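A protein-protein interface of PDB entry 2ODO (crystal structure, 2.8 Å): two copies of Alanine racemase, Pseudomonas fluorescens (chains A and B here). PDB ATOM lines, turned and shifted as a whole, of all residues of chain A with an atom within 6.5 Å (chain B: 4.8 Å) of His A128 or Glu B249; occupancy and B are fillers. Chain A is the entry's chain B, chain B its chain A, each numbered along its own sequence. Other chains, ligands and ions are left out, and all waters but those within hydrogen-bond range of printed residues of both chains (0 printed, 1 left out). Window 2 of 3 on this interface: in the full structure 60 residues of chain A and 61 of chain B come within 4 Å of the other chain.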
ATOM      1  N   KCX A 122     -12.919 -21.742  13.688  1.00  0.00           N
ATOM      2  CA  KCX A 122     -13.755 -21.510  14.863  1.00  0.00           C
ATOM      3  CB  KCX A 122     -14.772 -22.643  15.039  1.00  0.00           C
ATOM      4  CG  KCX A 122     -15.917 -22.310  15.984  1.00  0.00           C
ATOM      5  CD  KCX A 122     -17.108 -23.230  15.761  1.00  0.00           C
ATOM      6  CE  KCX A 122     -18.298 -22.813  16.617  1.00  0.00           C
ATOM      7  NZ  KCX A 122     -18.172 -23.245  18.044  1.00  0.00           N
ATOM      8  C   KCX A 122     -12.942 -21.307  16.141  1.00  0.00           C
ATOM      9  O   KCX A 122     -12.055 -22.100  16.466  1.00  0.00           O
ATOM     10  CX  KCX A 122     -18.961 -24.192  18.557  1.00  0.00           C
ATOM     11  OQ1 KCX A 122     -19.829 -24.747  17.865  1.00  0.00           O
ATOM     12  OQ2 KCX A 122     -18.827 -24.527  19.742  1.00  0.00           O
ATOM     13  N   ASP A 124     -13.031 -20.912  20.286  1.00  0.00           N
ATOM     14  CA  ASP A 124     -13.729 -21.068  21.552  1.00  0.00           C
ATOM     15  C   ASP A 124     -13.548 -19.776  22.349  1.00  0.00           C
ATOM     16  O   ASP A 124     -12.472 -19.509  22.896  1.00  0.00           O
ATOM     17  CB  ASP A 124     -13.196 -22.284  22.321  1.00  0.00           C
ATOM     18  CG  ASP A 124     -13.746 -22.380  23.738  1.00  0.00           C
ATOM     19  OD1 ASP A 124     -14.872 -21.900  23.997  1.00  0.00           O
ATOM     20  OD2 ASP A 124     -13.041 -22.948  24.595  1.00  0.00           O
ATOM     21  N   SER A 125     -14.606 -18.971  22.392  1.00  0.00           N
ATOM     22  CA  SER A 125     -14.557 -17.661  23.039  1.00  0.00           C
ATOM     23  C   SER A 125     -15.136 -17.665  24.457  1.00  0.00           C
ATOM     24  O   SER A 125     -15.163 -16.627  25.123  1.00  0.00           O
ATOM     25  CB  SER A 125     -15.250 -16.605  22.172  1.00  0.00           C
ATOM     26  OG  SER A 125     -16.595 -16.957  21.904  1.00  0.00           O
ATOM     27  N   GLY A 126     -15.588 -18.829  24.917  1.00  0.00           N
ATOM     28  CA  GLY A 126     -16.096 -18.959  26.279  1.00  0.00           C
ATOM     29  C   GLY A 126     -17.162 -20.013  26.513  1.00  0.00           C
ATOM     30  O   GLY A 126     -17.505 -20.301  27.661  1.00  0.00           O
ATOM     31  N   MET A 127     -17.694 -20.585  25.435  1.00  0.00           N
ATOM     32  CA  MET A 127     -18.703 -21.638  25.547  1.00  0.00           C
ATOM     33  C   MET A 127     -18.069 -22.970  25.949  1.00  0.00           C
ATOM     34  O   MET A 127     -18.674 -23.758  26.679  1.00  0.00           O
ATOM     35  CB  MET A 127     -19.485 -21.784  24.240  1.00  0.00           C
ATOM     36  CG  MET A 127     -20.623 -22.787  24.314  1.00  0.00           C
ATOM     37  SD  MET A 127     -21.666 -22.777  22.855  1.00  0.00           S
ATOM     38  CE  MET A 127     -22.727 -24.176  23.201  1.00  0.00           C
ATOM     39  N   HIS A 128     -16.847 -23.199  25.469  1.00  0.00           N
ATOM     40  CA  HIS A 128     -16.079 -24.420  25.739  1.00  0.00           C
ATOM     41  C   HIS A 128     -16.720 -25.691  25.171  1.00  0.00           C
ATOM     42  O   HIS A 128     -16.668 -26.758  25.789  1.00  0.00           O
ATOM     43  CB  HIS A 128     -15.759 -24.568  27.237  1.00  0.00           C
ATOM     44  CG  HIS A 128     -14.957 -23.435  27.803  1.00  0.00           C
ATOM     45  ND1 HIS A 128     -13.805 -22.968  27.210  1.00  0.00           N
ATOM     46  CD2 HIS A 128     -15.134 -22.690  28.919  1.00  0.00           C
ATOM     47  CE1 HIS A 128     -13.313 -21.975  27.928  1.00  0.00           C
ATOM     48  NE2 HIS A 128     -14.100 -21.787  28.972  1.00  0.00           N
ATOM     49  N   ARG A 129     -17.327 -25.562  23.994  1.00  0.00           N
ATOM     50  CA  ARG A 129     -17.772 -26.716  23.222  1.00  0.00           C
ATOM     51  C   ARG A 129     -16.633 -27.089  22.270  1.00  0.00           C
ATOM     52  O   ARG A 129     -15.642 -27.683  22.699  1.00  0.00           O
ATOM     53  CB  ARG A 129     -19.080 -26.410  22.479  1.00  0.00           C
ATOM     54  CG  ARG A 129     -19.821 -27.641  21.962  1.00  0.00           C
ATOM     55  CD  ARG A 129     -21.252 -27.315  21.543  1.00  0.00           C
ATOM     56  NE  ARG A 129     -21.315 -26.475  20.347  1.00  0.00           N
ATOM     57  CZ  ARG A 129     -22.439 -26.092  19.747  1.00  0.00           C
ATOM     58  NH1 ARG A 129     -23.621 -26.467  20.219  1.00  0.00           N
ATOM     59  NH2 ARG A 129     -22.383 -25.327  18.665  1.00  0.00           N
ATOM     60  N   VAL A 130     -16.761 -26.727  20.996  1.00  0.00           N
ATOM     61  CA  VAL A 130     -15.671 -26.896  20.030  1.00  0.00           C
ATOM     62  C   VAL A 130     -15.088 -25.545  19.614  1.00  0.00           C
ATOM     63  O   VAL A 130     -15.786 -24.527  19.627  1.00  0.00           O
ATOM     64  CB  VAL A 130     -16.087 -27.729  18.782  1.00  0.00           C
ATOM     65  CG1 VAL A 130     -16.257 -29.196  19.147  1.00  0.00           C
ATOM     66  CG2 VAL A 130     -17.354 -27.180  18.137  1.00  0.00           C
ATOM     67  N   ALA A 160     -22.662 -18.699  24.064  1.00  0.00           N
ATOM     68  CA  ALA A 160     -23.198 -19.667  25.019  1.00  0.00           C
ATOM     69  C   ALA A 160     -24.536 -19.229  25.607  1.00  0.00           C
ATOM     70  O   ALA A 160     -25.442 -20.046  25.764  1.00  0.00           O
ATOM     71  CB  ALA A 160     -22.195 -19.923  26.133  1.00  0.00           C
ATOM     72  N   ARG A 169     -22.376 -12.047  29.198  1.00  0.00           N
ATOM     73  CA  ARG A 169     -21.466 -13.080  28.696  1.00  0.00           C
ATOM     74  C   ARG A 169     -21.188 -12.918  27.201  1.00  0.00           C
ATOM     75  O   ARG A 169     -20.073 -13.174  26.741  1.00  0.00           O
ATOM     76  CB  ARG A 169     -22.012 -14.482  28.997  1.00  0.00           C
ATOM     77  CG  ARG A 169     -21.057 -15.638  28.676  1.00  0.00           C
ATOM     78  CD  ARG A 169     -19.771 -15.567  29.495  1.00  0.00           C
ATOM     79  NE  ARG A 169     -18.852 -16.661  29.182  1.00  0.00           N
ATOM     80  CZ  ARG A 169     -17.595 -16.736  29.611  1.00  0.00           C
ATOM     81  NH1 ARG A 169     -17.087 -15.777  30.375  1.00  0.00           N
ATOM     82  NH2 ARG A 169     -16.840 -17.771  29.275  1.00  0.00           N
ATOM     83  N   GLN A 173     -17.588 -12.542  25.332  1.00  0.00           N
ATOM     84  CA  GLN A 173     -17.190 -13.430  24.243  1.00  0.00           C
ATOM     85  C   GLN A 173     -16.740 -12.660  23.001  1.00  0.00           C
ATOM     86  O   GLN A 173     -15.831 -13.098  22.294  1.00  0.00           O
ATOM     87  CB  GLN A 173     -18.318 -14.404  23.895  1.00  0.00           C
ATOM     88  CG  GLN A 173     -18.540 -15.492  24.939  1.00  0.00           C
ATOM     89  CD  GLN A 173     -19.380 -16.642  24.419  1.00  0.00           C
ATOM     90  OE1 GLN A 173     -20.555 -16.773  24.762  1.00  0.00           O
ATOM     91  NE2 GLN A 173     -18.782 -17.482  23.581  1.00  0.00           N
ATOM     92  N   ARG B 243     -10.493 -31.036  25.377  1.00  0.00           N
ATOM     93  CA  ARG B 243     -10.105 -29.743  25.937  1.00  0.00           C
ATOM     94  C   ARG B 243      -9.795 -29.849  27.427  1.00  0.00           C
ATOM     95  O   ARG B 243     -10.496 -30.544  28.164  1.00  0.00           O
ATOM     96  CB  ARG B 243     -11.222 -28.722  25.714  1.00  0.00           C
ATOM     97  CG  ARG B 243     -10.814 -27.270  25.924  1.00  0.00           C
ATOM     98  CD  ARG B 243     -11.996 -26.324  25.753  1.00  0.00           C
ATOM     99  NE  ARG B 243     -12.718 -26.551  24.502  1.00  0.00           N
ATOM    100  CZ  ARG B 243     -12.347 -26.081  23.312  1.00  0.00           C
ATOM    101  NH1 ARG B 243     -11.250 -25.345  23.187  1.00  0.00           N
ATOM    102  NH2 ARG B 243     -13.078 -26.350  22.240  1.00  0.00           N
ATOM    103  N   LEU B 245      -9.576 -27.768  30.937  1.00  0.00           N
ATOM    104  CA  LEU B 245     -10.101 -26.556  31.555  1.00  0.00           C
ATOM    105  C   LEU B 245      -9.704 -26.448  33.023  1.00  0.00           C
ATOM    106  O   LEU B 245      -9.692 -27.454  33.736  1.00  0.00           O
ATOM    107  CB  LEU B 245     -11.630 -26.503  31.433  1.00  0.00           C
ATOM    108  CG  LEU B 245     -12.277 -26.323  30.055  1.00  0.00           C
ATOM    109  CD1 LEU B 245     -13.782 -26.487  30.157  1.00  0.00           C
ATOM    110  CD2 LEU B 245     -11.928 -24.973  29.441  1.00  0.00           C
ATOM    111  N   PRO B 246      -9.368 -25.225  33.477  1.00  0.00           N
ATOM    112  CA  PRO B 246      -9.173 -24.976  34.905  1.00  0.00           C
ATOM    113  C   PRO B 246     -10.506 -24.926  35.658  1.00  0.00           C
ATOM    114  O   PRO B 246     -11.574 -25.018  35.041  1.00  0.00           O
ATOM    115  CB  PRO B 246      -8.493 -23.604  34.926  1.00  0.00           C
ATOM    116  CG  PRO B 246      -8.975 -22.932  33.696  1.00  0.00           C
ATOM    117  CD  PRO B 246      -9.129 -24.015  32.669  1.00  0.00           C
ATOM    118  N   ALA B 247     -10.435 -24.787  36.979  1.00  0.00           N
ATOM    119  CA  ALA B 247     -11.628 -24.682  37.816  1.00  0.00           C
ATOM    120  C   ALA B 247     -12.330 -23.348  37.596  1.00  0.00           C
ATOM    121  O   ALA B 247     -11.679 -22.317  37.412  1.00  0.00           O
ATOM    122  CB  ALA B 247     -11.265 -24.857  39.281  1.00  0.00           C
ATOM    123  N   GLY B 248     -13.660 -23.383  37.607  1.00  0.00           N
ATOM    124  CA  GLY B 248     -14.476 -22.178  37.472  1.00  0.00           C
ATOM    125  C   GLY B 248     -14.782 -21.776  36.041  1.00  0.00           C
ATOM    126  O   GLY B 248     -14.965 -20.591  35.753  1.00  0.00           O
ATOM    127  N   GLU B 249     -14.843 -22.760  35.146  1.00  0.00           N
ATOM    128  CA  GLU B 249     -15.144 -22.510  33.738  1.00  0.00           C
ATOM    129  C   GLU B 249     -16.522 -23.042  33.342  1.00  0.00           C
ATOM    130  O   GLU B 249     -16.855 -24.188  33.651  1.00  0.00           O
ATOM    131  CB  GLU B 249     -14.061 -23.102  32.829  1.00  0.00           C
ATOM    132  CG  GLU B 249     -12.739 -22.332  32.825  1.00  0.00           C
ATOM    133  CD  GLU B 249     -12.873 -20.896  32.331  1.00  0.00           C
ATOM    134  OE1 GLU B 249     -13.592 -20.660  31.337  1.00  0.00           O
ATOM    135  OE2 GLU B 249     -12.248 -20.003  32.940  1.00  0.00           O
ATOM    136  N   PRO B 250     -17.329 -22.207  32.657  1.00  0.00           N
ATOM    137  CA  PRO B 250     -18.660 -22.616  32.202  1.00  0.00           C
ATOM    138  C   PRO B 250     -18.602 -23.504  30.957  1.00  0.00           C
ATOM    139  O   PRO B 250     -17.803 -23.253  30.054  1.00  0.00           O
ATOM    140  CB  PRO B 250     -19.344 -21.284  31.884  1.00  0.00           C
ATOM    141  CG  PRO B 250     -18.235 -20.360  31.531  1.00  0.00           C
ATOM    142  CD  PRO B 250     -17.017 -20.813  32.285  1.00  0.00           C
ATOM    143  N   VAL B 251     -19.441 -24.536  30.918  1.00  0.00           N
ATOM    144  CA  VAL B 251     -19.449 -25.480  29.799  1.00  0.00           C
ATOM    145  C   VAL B 251     -20.837 -25.588  29.160  1.00  0.00           C
ATOM    146  O   VAL B 251     -21.812 -25.948  29.825  1.00  0.00           O
ATOM    147  CB  VAL B 251     -18.941 -26.891  30.221  1.00  0.00           C
ATOM    148  CG1 VAL B 251     -18.875 -27.827  29.020  1.00  0.00           C
ATOM    149  CG2 VAL B 251     -17.574 -26.803  30.891  1.00  0.00           C
ATOM    150  N   PHE B 257     -23.328 -25.821  33.803  1.00  0.00           N
ATOM    151  CA  PHE B 257     -22.281 -26.563  34.494  1.00  0.00           C
ATOM    152  C   PHE B 257     -20.975 -25.778  34.538  1.00  0.00           C
ATOM    153  O   PHE B 257     -20.413 -25.424  33.499  1.00  0.00           O
ATOM    154  CB  PHE B 257     -22.058 -27.940  33.862  1.00  0.00           C
ATOM    155  CG  PHE B 257     -20.946 -28.723  34.500  1.00  0.00           C
ATOM    156  CD1 PHE B 257     -21.131 -29.340  35.736  1.00  0.00           C
ATOM    157  CD2 PHE B 257     -19.709 -28.834  33.876  1.00  0.00           C
ATOM    158  CE1 PHE B 257     -20.102 -30.059  36.337  1.00  0.00           C
ATOM    159  CE2 PHE B 257     -18.678 -29.550  34.469  1.00  0.00           C
ATOM    160  CZ  PHE B 257     -18.874 -30.162  35.703  1.00  0.00           C
ATOM    161  N   ILE B 258     -20.505 -25.513  35.752  1.00  0.00           N
ATOM    162  CA  ILE B 258     -19.236 -24.825  35.973  1.00  0.00           C
ATOM    163  C   ILE B 258     -18.246 -25.803  36.604  1.00  0.00           C
ATOM    164  O   ILE B 258     -18.560 -26.447  37.607  1.00  0.00           O
ATOM    165  CB  ILE B 258     -19.405 -23.559  36.864  1.00  0.00           C
ATOM    166  CG1 ILE B 258     -20.242 -22.491  36.154  1.00  0.00           C
ATOM    167  CG2 ILE B 258     -18.056 -22.962  37.234  1.00  0.00           C
ATOM    168  CD1 ILE B 258     -21.704 -22.491  36.537  1.00  0.00           C
ATOM    169  N   THR B 259     -17.060 -25.908  36.004  1.00  0.00           N
ATOM    170  CA  THR B 259     -16.011 -26.818  36.471  1.00  0.00           C
ATOM    171  C   THR B 259     -15.691 -26.596  37.953  1.00  0.00           C
ATOM    172  O   THR B 259     -15.231 -25.515  38.331  1.00  0.00           O
ATOM    173  CB  THR B 259     -14.707 -26.684  35.634  1.00  0.00           C
ATOM    174  OG1 THR B 259     -14.195 -25.348  35.736  1.00  0.00           O
ATOM    175  CG2 THR B 259     -14.958 -27.007  34.167  1.00  0.00           C
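O of Arg A129 is in hydrogen-bond range of NH2 of Arg B243, 2.9 Å away.
The side-chain carboxylate (OE1) of Glu B249 is in hydrogen-bond range of a ring nitrogen (NE2) of His A128 (2.7 Å).
The side-chain carboxylate (OD2) of Asp A124 is in salt-bridge range of the guanidinium group (NH1) of Arg B243 (3.3 Å).
O of Phe B257 is in hydrogen-bond range of N of Val B251 (2.9 Å).
A ring nitrogen (ND1) of His A128 sits at hydrogen-bond distance from the side-chain carboxylate (OD2) of Asp A124, at 2.7 Å.
NH2 of Arg A169 is in hydrogen-bond range of O of Gly A126, at 3.1 Å.
The backbone NH of Glu B249 sits at hydrogen-bond distance from the side-chain hydroxyl of Thr B259 (2.7 Å).
The side-chain carboxylate of Asp A124 sits at hydrogen-bond distance from the backbone NH of Gly A126, at 3.3 Å.
OQ1 of KCX A122 lies close to the guanidinium group (NH2) of Arg A129, 2.7 Å away.
Among the printed residues, pairs that only touch across the chains: Gly A126 with Pro B250 (3.8 Å), Met A127 with Pro B250 (3.5 Å), Met A127 with Val B251 (3.6 Å), His A128 with Leu B245 (3.5 Å), His A128 with Pro B250 (3.0 Å), Val A130 with Arg B243 (3.4 Å) and Arg A169 with Pro B250 (3.7 Å).
His A128 touches three residues of chain B.
Printed residues of chain B within 4 Å of Arg A169: Pro B250 (3.7 Å).
Printed residues of chain A within 4 Å of Val B251: Met A127.
Of the printed residues of chain A, Arg B243 touches Asp A124 (3.3 Å), Arg A129 (2.9 Å) and Val A130 (3.4 Å).
Gly B248 touches none of the printed residues of chain A.
Gln A173 touches none of the printed residues of chain B.
The nearest residue of chain A that does not touch Glu B249 is Arg A169 (4.8 Å).
The nearest printed residue of chain A that does not touch Arg B243 is His A128 (4.1 Å).
Printed residues of chain B that touch a printed residue of chain A: Arg B243, Leu B245, Glu B249, Pro B250 and Val B251.
Hydrophobic or aromatic side chains of chain B that line the printed part of chain A: Leu B245 and Pro B250.
Of the 11 printed residues of chain A, 7 touch a printed residue of chain B.
Printed residues of chain A that touch a printed residue of chain B: Asp A124, Gly A126, Met A127, His A128, Arg A129, Val A130 and Arg A169.
Hydrophobic or aromatic side chains of chain A that line the printed part of chain B: His A128.
Among the printed residues, 10 pairs touch across the chains.
Among the printed residues, Asp or Glu carboxylates within 4 Å of a Lys or Arg side-chain nitrogen of the other chain: Asp A124 with Arg B243 (3.3 Å).
No position is printed for both chains.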
